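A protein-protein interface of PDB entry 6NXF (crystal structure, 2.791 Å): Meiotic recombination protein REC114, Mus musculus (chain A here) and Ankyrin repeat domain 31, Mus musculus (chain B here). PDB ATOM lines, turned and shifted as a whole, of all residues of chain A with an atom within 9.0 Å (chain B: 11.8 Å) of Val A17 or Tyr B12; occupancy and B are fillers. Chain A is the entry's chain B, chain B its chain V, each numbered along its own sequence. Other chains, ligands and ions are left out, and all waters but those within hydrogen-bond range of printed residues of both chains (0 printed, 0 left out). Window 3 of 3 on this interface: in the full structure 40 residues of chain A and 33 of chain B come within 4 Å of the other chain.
N of Lys B16 sits at hydrogen-bond distance from O of Gln A79 (2.8 Å).
N of Val A64 is in hydrogen-bond range of O of Ser A76 (2.9 Å). The backbone carbonyl oxygen of Phe A74 is in hydrogen-bond range of the backbone NH of Thr A66. O of His B11 sits at hydrogen-bond distance from NE2 of Gln B14.
Among the printed residues, pairs that only touch across the chains: Val A17 with Tyr B12 (3.1 Å), Gln A19 with Leu B13 (3.7 Å), Thr A66 with Leu B13 (3.99 Å), Val A68 with Pro B10 (3.5 Å), Val A68 with Tyr B12 (3.4 Å), His A72 with Thr B8 (3.7 Å), Phe A74 with Thr B8 (3.5 Å), Phe A74 with Pro B10 (3.5 Å), Phe A74 with Leu B13 (3.8 Å), Ser A76 with Ile B15 (3.9 Å), Gly A78 with Gln B14 (3.9 Å), Gln A79 with Gln B14 (3.0 Å) and Gln A79 with Ile B15 (3.7 Å).
Val A17 touches just one residue of chain B: Tyr B12 (3.1 Å). No residue of chain B comes within 4 Å of Ser A18. Gln A19 touches just one residue of chain B: Leu B13 (3.7 Å). Of the printed residues of chain B, Val A68 touches Pro B10 and Tyr B12. His B11 touches none of the printed residues of chain A. Printed residues of chain A within 4 Å of Gln B14: Gly A78 and Gln A79. Printed residues of chain B within 4 Å of Gly A78: Gln B14 (3.9 Å). The nearest printed residue of chain B that does not touch Gln A79 is Leu B13 (5.6 Å).
Of the 18 printed residues of chain A, 9 touch a printed residue of chain B. Hydrophobic or aromatic side chains of chain A within 4 Å of the printed part of chain B: Val A17, Val A68, His A72 and Phe A74. Of the 9 printed residues of chain B, 7 touch a printed residue of chain A.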
ATOM      1  N   VAL A  17     -20.907  10.704  -6.685  1.00  0.00           N
ATOM      2  CA  VAL A  17     -20.055  11.076  -5.547  1.00  0.00           C
ATOM      3  C   VAL A  17     -20.812  11.051  -4.220  1.00  0.00           C
ATOM      4  O   VAL A  17     -21.684  11.888  -3.959  1.00  0.00           O
ATOM      5  CB  VAL A  17     -19.410  12.463  -5.764  1.00  0.00           C
ATOM      6  CG1 VAL A  17     -18.686  12.950  -4.484  1.00  0.00           C
ATOM      7  CG2 VAL A  17     -18.449  12.389  -6.933  1.00  0.00           C
ATOM      8  N   SER A  18     -20.463  10.085  -3.379  1.00  0.00           N
ATOM      9  CA  SER A  18     -21.080   9.940  -2.076  1.00  0.00           C
ATOM     10  C   SER A  18     -20.002  10.043  -1.007  1.00  0.00           C
ATOM     11  O   SER A  18     -18.945   9.419  -1.119  1.00  0.00           O
ATOM     12  CB  SER A  18     -21.858   8.627  -1.984  1.00  0.00           C
ATOM     13  OG  SER A  18     -23.210   8.818  -2.397  1.00  0.00           O
ATOM     14  N   GLN A  19     -20.256  10.875  -0.005  1.00  0.00           N
ATOM     15  CA  GLN A  19     -19.399  11.047   1.149  1.00  0.00           C
ATOM     16  C   GLN A  19     -20.228  10.813   2.399  1.00  0.00           C
ATOM     17  O   GLN A  19     -21.428  11.105   2.419  1.00  0.00           O
ATOM     18  CB  GLN A  19     -18.813  12.450   1.234  1.00  0.00           C
ATOM     19  CG  GLN A  19     -18.149  13.005  -0.009  1.00  0.00           C
ATOM     20  CD  GLN A  19     -17.605  14.409   0.264  1.00  0.00           C
ATOM     21  OE1 GLN A  19     -18.061  15.083   1.189  1.00  0.00           O
ATOM     22  NE2 GLN A  19     -16.620  14.843  -0.516  1.00  0.00           N
ATOM     23  N   TRP A  20     -19.573  10.305   3.446  1.00  0.00           N
ATOM     24  CA  TRP A  20     -20.163  10.118   4.764  1.00  0.00           C
ATOM     25  C   TRP A  20     -19.317  10.828   5.817  1.00  0.00           C
ATOM     26  O   TRP A  20     -18.087  10.915   5.700  1.00  0.00           O
ATOM     27  CB  TRP A  20     -20.263   8.653   5.131  1.00  0.00           C
ATOM     28  CG  TRP A  20     -21.049   7.788   4.198  1.00  0.00           C
ATOM     29  CD1 TRP A  20     -22.276   7.229   4.434  1.00  0.00           C
ATOM     30  CD2 TRP A  20     -20.647   7.335   2.903  1.00  0.00           C
ATOM     31  NE1 TRP A  20     -22.666   6.466   3.361  1.00  0.00           N
ATOM     32  CE2 TRP A  20     -21.684   6.516   2.406  1.00  0.00           C
ATOM     33  CE3 TRP A  20     -19.514   7.544   2.111  1.00  0.00           C
ATOM     34  CZ2 TRP A  20     -21.622   5.910   1.154  1.00  0.00           C
ATOM     35  CZ3 TRP A  20     -19.456   6.946   0.868  1.00  0.00           C
ATOM     36  CH2 TRP A  20     -20.502   6.137   0.403  1.00  0.00           C
ATOM     37  N   VAL A  64     -14.046  13.229   6.998  1.00  0.00           N
ATOM     38  CA  VAL A  64     -14.963  12.878   5.921  1.00  0.00           C
ATOM     39  C   VAL A  64     -14.320  11.810   5.045  1.00  0.00           C
ATOM     40  O   VAL A  64     -13.234  12.021   4.490  1.00  0.00           O
ATOM     41  CB  VAL A  64     -15.367  14.101   5.072  1.00  0.00           C
ATOM     42  CG1 VAL A  64     -14.136  14.869   4.613  1.00  0.00           C
ATOM     43  CG2 VAL A  64     -16.183  13.661   3.881  1.00  0.00           C
ATOM     44  N   LEU A  65     -14.996  10.677   4.907  1.00  0.00           N
ATOM     45  CA  LEU A  65     -14.629   9.639   3.955  1.00  0.00           C
ATOM     46  C   LEU A  65     -15.460   9.792   2.686  1.00  0.00           C
ATOM     47  O   LEU A  65     -16.686   9.895   2.754  1.00  0.00           O
ATOM     48  CB  LEU A  65     -14.855   8.261   4.575  1.00  0.00           C
ATOM     49  CG  LEU A  65     -14.843   6.929   3.809  1.00  0.00           C
ATOM     50  CD1 LEU A  65     -14.636   5.753   4.781  1.00  0.00           C
ATOM     51  CD2 LEU A  65     -16.129   6.731   3.032  1.00  0.00           C
ATOM     52  N   THR A  66     -14.803   9.753   1.529  1.00  0.00           N
ATOM     53  CA  THR A  66     -15.496   9.887   0.254  1.00  0.00           C
ATOM     54  C   THR A  66     -15.075   8.783  -0.710  1.00  0.00           C
ATOM     55  O   THR A  66     -13.936   8.311  -0.680  1.00  0.00           O
ATOM     56  CB  THR A  66     -15.229  11.259  -0.375  1.00  0.00           C
ATOM     57  OG1 THR A  66     -14.375  11.106  -1.513  1.00  0.00           O
ATOM     58  CG2 THR A  66     -14.578  12.209   0.652  1.00  0.00           C
ATOM     59  N   ILE A  67     -16.002   8.392  -1.585  1.00  0.00           N
ATOM     60  CA  ILE A  67     -15.780   7.327  -2.561  1.00  0.00           C
ATOM     61  C   ILE A  67     -16.171   7.833  -3.947  1.00  0.00           C
ATOM     62  O   ILE A  67     -17.359   8.020  -4.235  1.00  0.00           O
ATOM     63  CB  ILE A  67     -16.566   6.059  -2.215  1.00  0.00           C
ATOM     64  CG1 ILE A  67     -15.969   5.374  -0.993  1.00  0.00           C
ATOM     65  CG2 ILE A  67     -16.563   5.095  -3.368  1.00  0.00           C
ATOM     66  CD1 ILE A  67     -16.548   3.992  -0.772  1.00  0.00           C
ATOM     67  N   VAL A  68     -15.179   8.026  -4.814  1.00  0.00           N
ATOM     68  CA  VAL A  68     -15.402   8.545  -6.160  1.00  0.00           C
ATOM     69  C   VAL A  68     -15.986   7.443  -7.027  1.00  0.00           C
ATOM     70  O   VAL A  68     -15.756   6.253  -6.787  1.00  0.00           O
ATOM     71  CB  VAL A  68     -14.077   9.093  -6.731  1.00  0.00           C
ATOM     72  CG1 VAL A  68     -14.104   9.231  -8.241  1.00  0.00           C
ATOM     73  CG2 VAL A  68     -13.764  10.427  -6.108  1.00  0.00           C
ATOM     74  N   VAL A  69     -16.771   7.836  -8.030  1.00  0.00           N
ATOM     75  CA  VAL A  69     -17.352   6.853  -8.940  1.00  0.00           C
ATOM     76  C   VAL A  69     -16.258   6.045  -9.623  1.00  0.00           C
ATOM     77  O   VAL A  69     -16.417   4.836  -9.837  1.00  0.00           O
ATOM     78  CB  VAL A  69     -18.275   7.539  -9.963  1.00  0.00           C
ATOM     79  CG1 VAL A  69     -18.986   6.476 -10.810  1.00  0.00           C
ATOM     80  CG2 VAL A  69     -19.271   8.484  -9.234  1.00  0.00           C
ATOM     81  N   SER A  70     -15.124   6.690  -9.948  1.00  0.00           N
ATOM     82  CA  SER A  70     -13.982   5.976 -10.524  1.00  0.00           C
ATOM     83  C   SER A  70     -13.666   4.717  -9.742  1.00  0.00           C
ATOM     84  O   SER A  70     -13.507   3.635 -10.318  1.00  0.00           O
ATOM     85  CB  SER A  70     -12.743   6.869 -10.556  1.00  0.00           C
ATOM     86  OG  SER A  70     -12.959   8.029 -11.334  1.00  0.00           O
ATOM     87  N   GLY A  71     -13.594   4.835  -8.427  1.00  0.00           N
ATOM     88  CA  GLY A  71     -13.281   3.707  -7.587  1.00  0.00           C
ATOM     89  C   GLY A  71     -12.250   4.103  -6.555  1.00  0.00           C
ATOM     90  O   GLY A  71     -11.634   3.235  -5.916  1.00  0.00           O
ATOM     91  N   HIS A  72     -12.064   5.409  -6.364  1.00  0.00           N
ATOM     92  CA  HIS A  72     -11.070   5.885  -5.415  1.00  0.00           C
ATOM     93  C   HIS A  72     -11.690   6.191  -4.067  1.00  0.00           C
ATOM     94  O   HIS A  72     -12.848   6.608  -3.966  1.00  0.00           O
ATOM     95  CB  HIS A  72     -10.358   7.118  -5.926  1.00  0.00           C
ATOM     96  CG  HIS A  72      -9.576   6.874  -7.169  1.00  0.00           C
ATOM     97  ND1 HIS A  72      -9.941   5.928  -8.102  1.00  0.00           N
ATOM     98  CD2 HIS A  72      -8.443   7.449  -7.634  1.00  0.00           C
ATOM     99  CE1 HIS A  72      -9.067   5.935  -9.093  1.00  0.00           C
ATOM    100  NE2 HIS A  72      -8.150   6.853  -8.833  1.00  0.00           N
ATOM    101  N   PHE A  74     -10.962   7.939  -0.118  1.00  0.00           N
ATOM    102  CA  PHE A  74     -10.195   8.887   0.677  1.00  0.00           C
ATOM    103  C   PHE A  74     -10.806   9.078   2.050  1.00  0.00           C
ATOM    104  O   PHE A  74     -12.008   8.913   2.257  1.00  0.00           O
ATOM    105  CB  PHE A  74     -10.117  10.261   0.043  1.00  0.00           C
ATOM    106  CG  PHE A  74      -9.710  10.251  -1.384  1.00  0.00           C
ATOM    107  CD1 PHE A  74      -8.391  10.453  -1.733  1.00  0.00           C
ATOM    108  CD2 PHE A  74     -10.641  10.069  -2.371  1.00  0.00           C
ATOM    109  CE1 PHE A  74      -8.001  10.450  -3.039  1.00  0.00           C
ATOM    110  CE2 PHE A  74     -10.259  10.079  -3.698  1.00  0.00           C
ATOM    111  CZ  PHE A  74      -8.939  10.269  -4.027  1.00  0.00           C
ATOM    112  N   SER A  76     -10.252  12.303   4.871  1.00  0.00           N
ATOM    113  CA  SER A  76      -9.638  13.619   4.988  1.00  0.00           C
ATOM    114  C   SER A  76     -10.212  14.336   6.199  1.00  0.00           C
ATOM    115  O   SER A  76     -11.372  14.129   6.570  1.00  0.00           O
ATOM    116  CB  SER A  76      -9.866  14.447   3.714  1.00  0.00           C
ATOM    117  OG  SER A  76     -11.059  14.026   3.076  1.00  0.00           O
ATOM    118  N   GLY A  78     -10.412  18.214   6.899  1.00  0.00           N
ATOM    119  CA  GLY A  78     -10.131  19.527   6.374  1.00  0.00           C
ATOM    120  C   GLY A  78      -9.264  19.398   5.152  1.00  0.00           C
ATOM    121  O   GLY A  78      -9.646  18.781   4.152  1.00  0.00           O
ATOM    122  N   GLN A  79      -8.075  19.979   5.222  1.00  0.00           N
ATOM    123  CA  GLN A  79      -7.217  20.076   4.060  1.00  0.00           C
ATOM    124  C   GLN A  79      -6.082  19.076   4.103  1.00  0.00           C
ATOM    125  O   GLN A  79      -5.126  19.182   3.322  1.00  0.00           O
ATOM    126  CB  GLN A  79      -6.665  21.483   3.931  1.00  0.00           C
ATOM    127  CG  GLN A  79      -7.131  22.109   2.635  1.00  0.00           C
ATOM    128  CD  GLN A  79      -7.879  23.431   2.809  1.00  0.00           C
ATOM    129  OE1 GLN A  79      -7.329  24.497   2.516  1.00  0.00           O
ATOM    130  NE2 GLN A  79      -9.142  23.365   3.260  1.00  0.00           N
ATOM    131  N   THR A 138     -21.982   0.910  -0.836  1.00  0.00           N
ATOM    132  CA  THR A 138     -21.192   1.555  -1.883  1.00  0.00           C
ATOM    133  C   THR A 138     -19.840   0.875  -2.076  1.00  0.00           C
ATOM    134  O   THR A 138     -19.306   0.850  -3.188  1.00  0.00           O
ATOM    135  CB  THR A 138     -20.999   3.041  -1.556  1.00  0.00           C
ATOM    136  OG1 THR A 138     -22.278   3.687  -1.472  1.00  0.00           O
ATOM    137  CG2 THR A 138     -20.165   3.740  -2.629  1.00  0.00           C
ATOM    138  N   THR B   8      -3.747  10.767  -7.458  1.00  0.00           N
ATOM    139  CA  THR B   8      -4.937  11.411  -8.007  1.00  0.00           C
ATOM    140  C   THR B   8      -5.856  11.828  -6.874  1.00  0.00           C
ATOM    141  O   THR B   8      -6.227  10.990  -6.049  1.00  0.00           O
ATOM    142  CB  THR B   8      -5.689  10.479  -8.957  1.00  0.00           C
ATOM    143  OG1 THR B   8      -5.246  10.725 -10.292  1.00  0.00           O
ATOM    144  CG2 THR B   8      -7.224  10.690  -8.869  1.00  0.00           C
ATOM    145  N   ILE B   9      -6.222  13.109  -6.835  1.00  0.00           N
ATOM    146  CA  ILE B   9      -7.187  13.613  -5.860  1.00  0.00           C
ATOM    147  C   ILE B   9      -8.206  14.476  -6.590  1.00  0.00           C
ATOM    148  O   ILE B   9      -7.818  15.428  -7.293  1.00  0.00           O
ATOM    149  CB  ILE B   9      -6.504  14.424  -4.741  1.00  0.00           C
ATOM    150  CG1 ILE B   9      -5.099  13.864  -4.429  1.00  0.00           C
ATOM    151  CG2 ILE B   9      -7.397  14.478  -3.541  1.00  0.00           C
ATOM    152  CD1 ILE B   9      -4.672  13.805  -2.937  1.00  0.00           C
ATOM    153  N   PRO B  10      -9.507  14.207  -6.453  1.00  0.00           N
ATOM    154  CA  PRO B  10     -10.512  15.088  -7.071  1.00  0.00           C
ATOM    155  C   PRO B  10     -10.337  16.513  -6.579  1.00  0.00           C
ATOM    156  O   PRO B  10      -9.791  16.755  -5.498  1.00  0.00           O
ATOM    157  CB  PRO B  10     -11.850  14.508  -6.593  1.00  0.00           C
ATOM    158  CG  PRO B  10     -11.559  13.160  -6.180  1.00  0.00           C
ATOM    159  CD  PRO B  10     -10.135  13.180  -5.624  1.00  0.00           C
ATOM    160  N   HIS B  11     -10.797  17.467  -7.386  1.00  0.00           N
ATOM    161  CA  HIS B  11     -10.538  18.858  -7.040  1.00  0.00           C
ATOM    162  C   HIS B  11     -11.426  19.322  -5.897  1.00  0.00           C
ATOM    163  O   HIS B  11     -10.999  20.159  -5.090  1.00  0.00           O
ATOM    164  CB  HIS B  11     -10.737  19.751  -8.251  1.00  0.00           C
ATOM    165  CG  HIS B  11     -12.168  19.907  -8.647  1.00  0.00           C
ATOM    166  ND1 HIS B  11     -12.900  18.882  -9.219  1.00  0.00           N
ATOM    167  CD2 HIS B  11     -13.009  20.962  -8.544  1.00  0.00           C
ATOM    168  CE1 HIS B  11     -14.130  19.301  -9.454  1.00  0.00           C
ATOM    169  NE2 HIS B  11     -14.220  20.561  -9.059  1.00  0.00           N
ATOM    170  N   TYR B  12     -12.637  18.762  -5.779  1.00  0.00           N
ATOM    171  CA  TYR B  12     -13.548  19.192  -4.726  1.00  0.00           C
ATOM    172  C   TYR B  12     -13.149  18.727  -3.344  1.00  0.00           C
ATOM    173  O   TYR B  12     -13.838  19.067  -2.384  1.00  0.00           O
ATOM    174  CB  TYR B  12     -14.970  18.725  -4.996  1.00  0.00           C
ATOM    175  CG  TYR B  12     -15.095  17.287  -5.387  1.00  0.00           C
ATOM    176  CD1 TYR B  12     -15.233  16.287  -4.423  1.00  0.00           C
ATOM    177  CD2 TYR B  12     -15.106  16.913  -6.723  1.00  0.00           C
ATOM    178  CE1 TYR B  12     -15.367  14.941  -4.788  1.00  0.00           C
ATOM    179  CE2 TYR B  12     -15.238  15.583  -7.090  1.00  0.00           C
ATOM    180  CZ  TYR B  12     -15.363  14.610  -6.121  1.00  0.00           C
ATOM    181  OH  TYR B  12     -15.488  13.309  -6.510  1.00  0.00           O
ATOM    182  N   LEU B  13     -12.083  17.962  -3.170  1.00  0.00           N
ATOM    183  CA  LEU B  13     -11.740  17.632  -1.793  1.00  0.00           C
ATOM    184  C   LEU B  13     -10.935  18.743  -1.155  1.00  0.00           C
ATOM    185  O   LEU B  13     -11.029  18.943   0.058  1.00  0.00           O
ATOM    186  CB  LEU B  13     -10.990  16.303  -1.725  1.00  0.00           C
ATOM    187  CG  LEU B  13     -11.774  15.070  -1.251  1.00  0.00           C
ATOM    188  CD1 LEU B  13     -13.194  15.046  -1.787  1.00  0.00           C
ATOM    189  CD2 LEU B  13     -11.047  13.789  -1.649  1.00  0.00           C
ATOM    190  N   GLN B  14     -10.169  19.488  -1.953  1.00  0.00           N
ATOM    191  CA  GLN B  14      -9.363  20.608  -1.464  1.00  0.00           C
ATOM    192  C   GLN B  14      -8.341  20.093  -0.465  1.00  0.00           C
ATOM    193  O   GLN B  14      -8.502  20.240   0.750  1.00  0.00           O
ATOM    194  CB  GLN B  14     -10.234  21.709  -0.849  1.00  0.00           C
ATOM    195  CG  GLN B  14     -11.456  22.103  -1.690  1.00  0.00           C
ATOM    196  CD  GLN B  14     -11.111  22.986  -2.883  1.00  0.00           C
ATOM    197  OE1 GLN B  14     -10.151  23.761  -2.837  1.00  0.00           O
ATOM    198  NE2 GLN B  14     -11.911  22.883  -3.958  1.00  0.00           N
ATOM    199  N   ILE B  15      -7.302  19.451  -0.979  1.00  0.00           N
ATOM    200  CA  ILE B  15      -6.278  18.817  -0.167  1.00  0.00           C
ATOM    201  C   ILE B  15      -5.002  19.603  -0.369  1.00  0.00           C
ATOM    202  O   ILE B  15      -4.584  19.835  -1.510  1.00  0.00           O
ATOM    203  CB  ILE B  15      -6.063  17.336  -0.548  1.00  0.00           C
ATOM    204  CG1 ILE B  15      -7.279  16.462  -0.193  1.00  0.00           C
ATOM    205  CG2 ILE B  15      -4.750  16.807   0.043  1.00  0.00           C
ATOM    206  CD1 ILE B  15      -7.741  16.572   1.247  1.00  0.00           C
ATOM    207  N   LYS B  16      -4.391  20.014   0.728  1.00  0.00           N
ATOM    208  CA  LYS B  16      -3.120  20.695   0.673  1.00  0.00           C
ATOM    209  C   LYS B  16      -2.009  19.918   1.332  1.00  0.00           C
ATOM    210  O   LYS B  16      -0.857  20.047   0.917  1.00  0.00           O
ATOM    211  CB  LYS B  16      -3.231  22.072   1.333  1.00  0.00           C
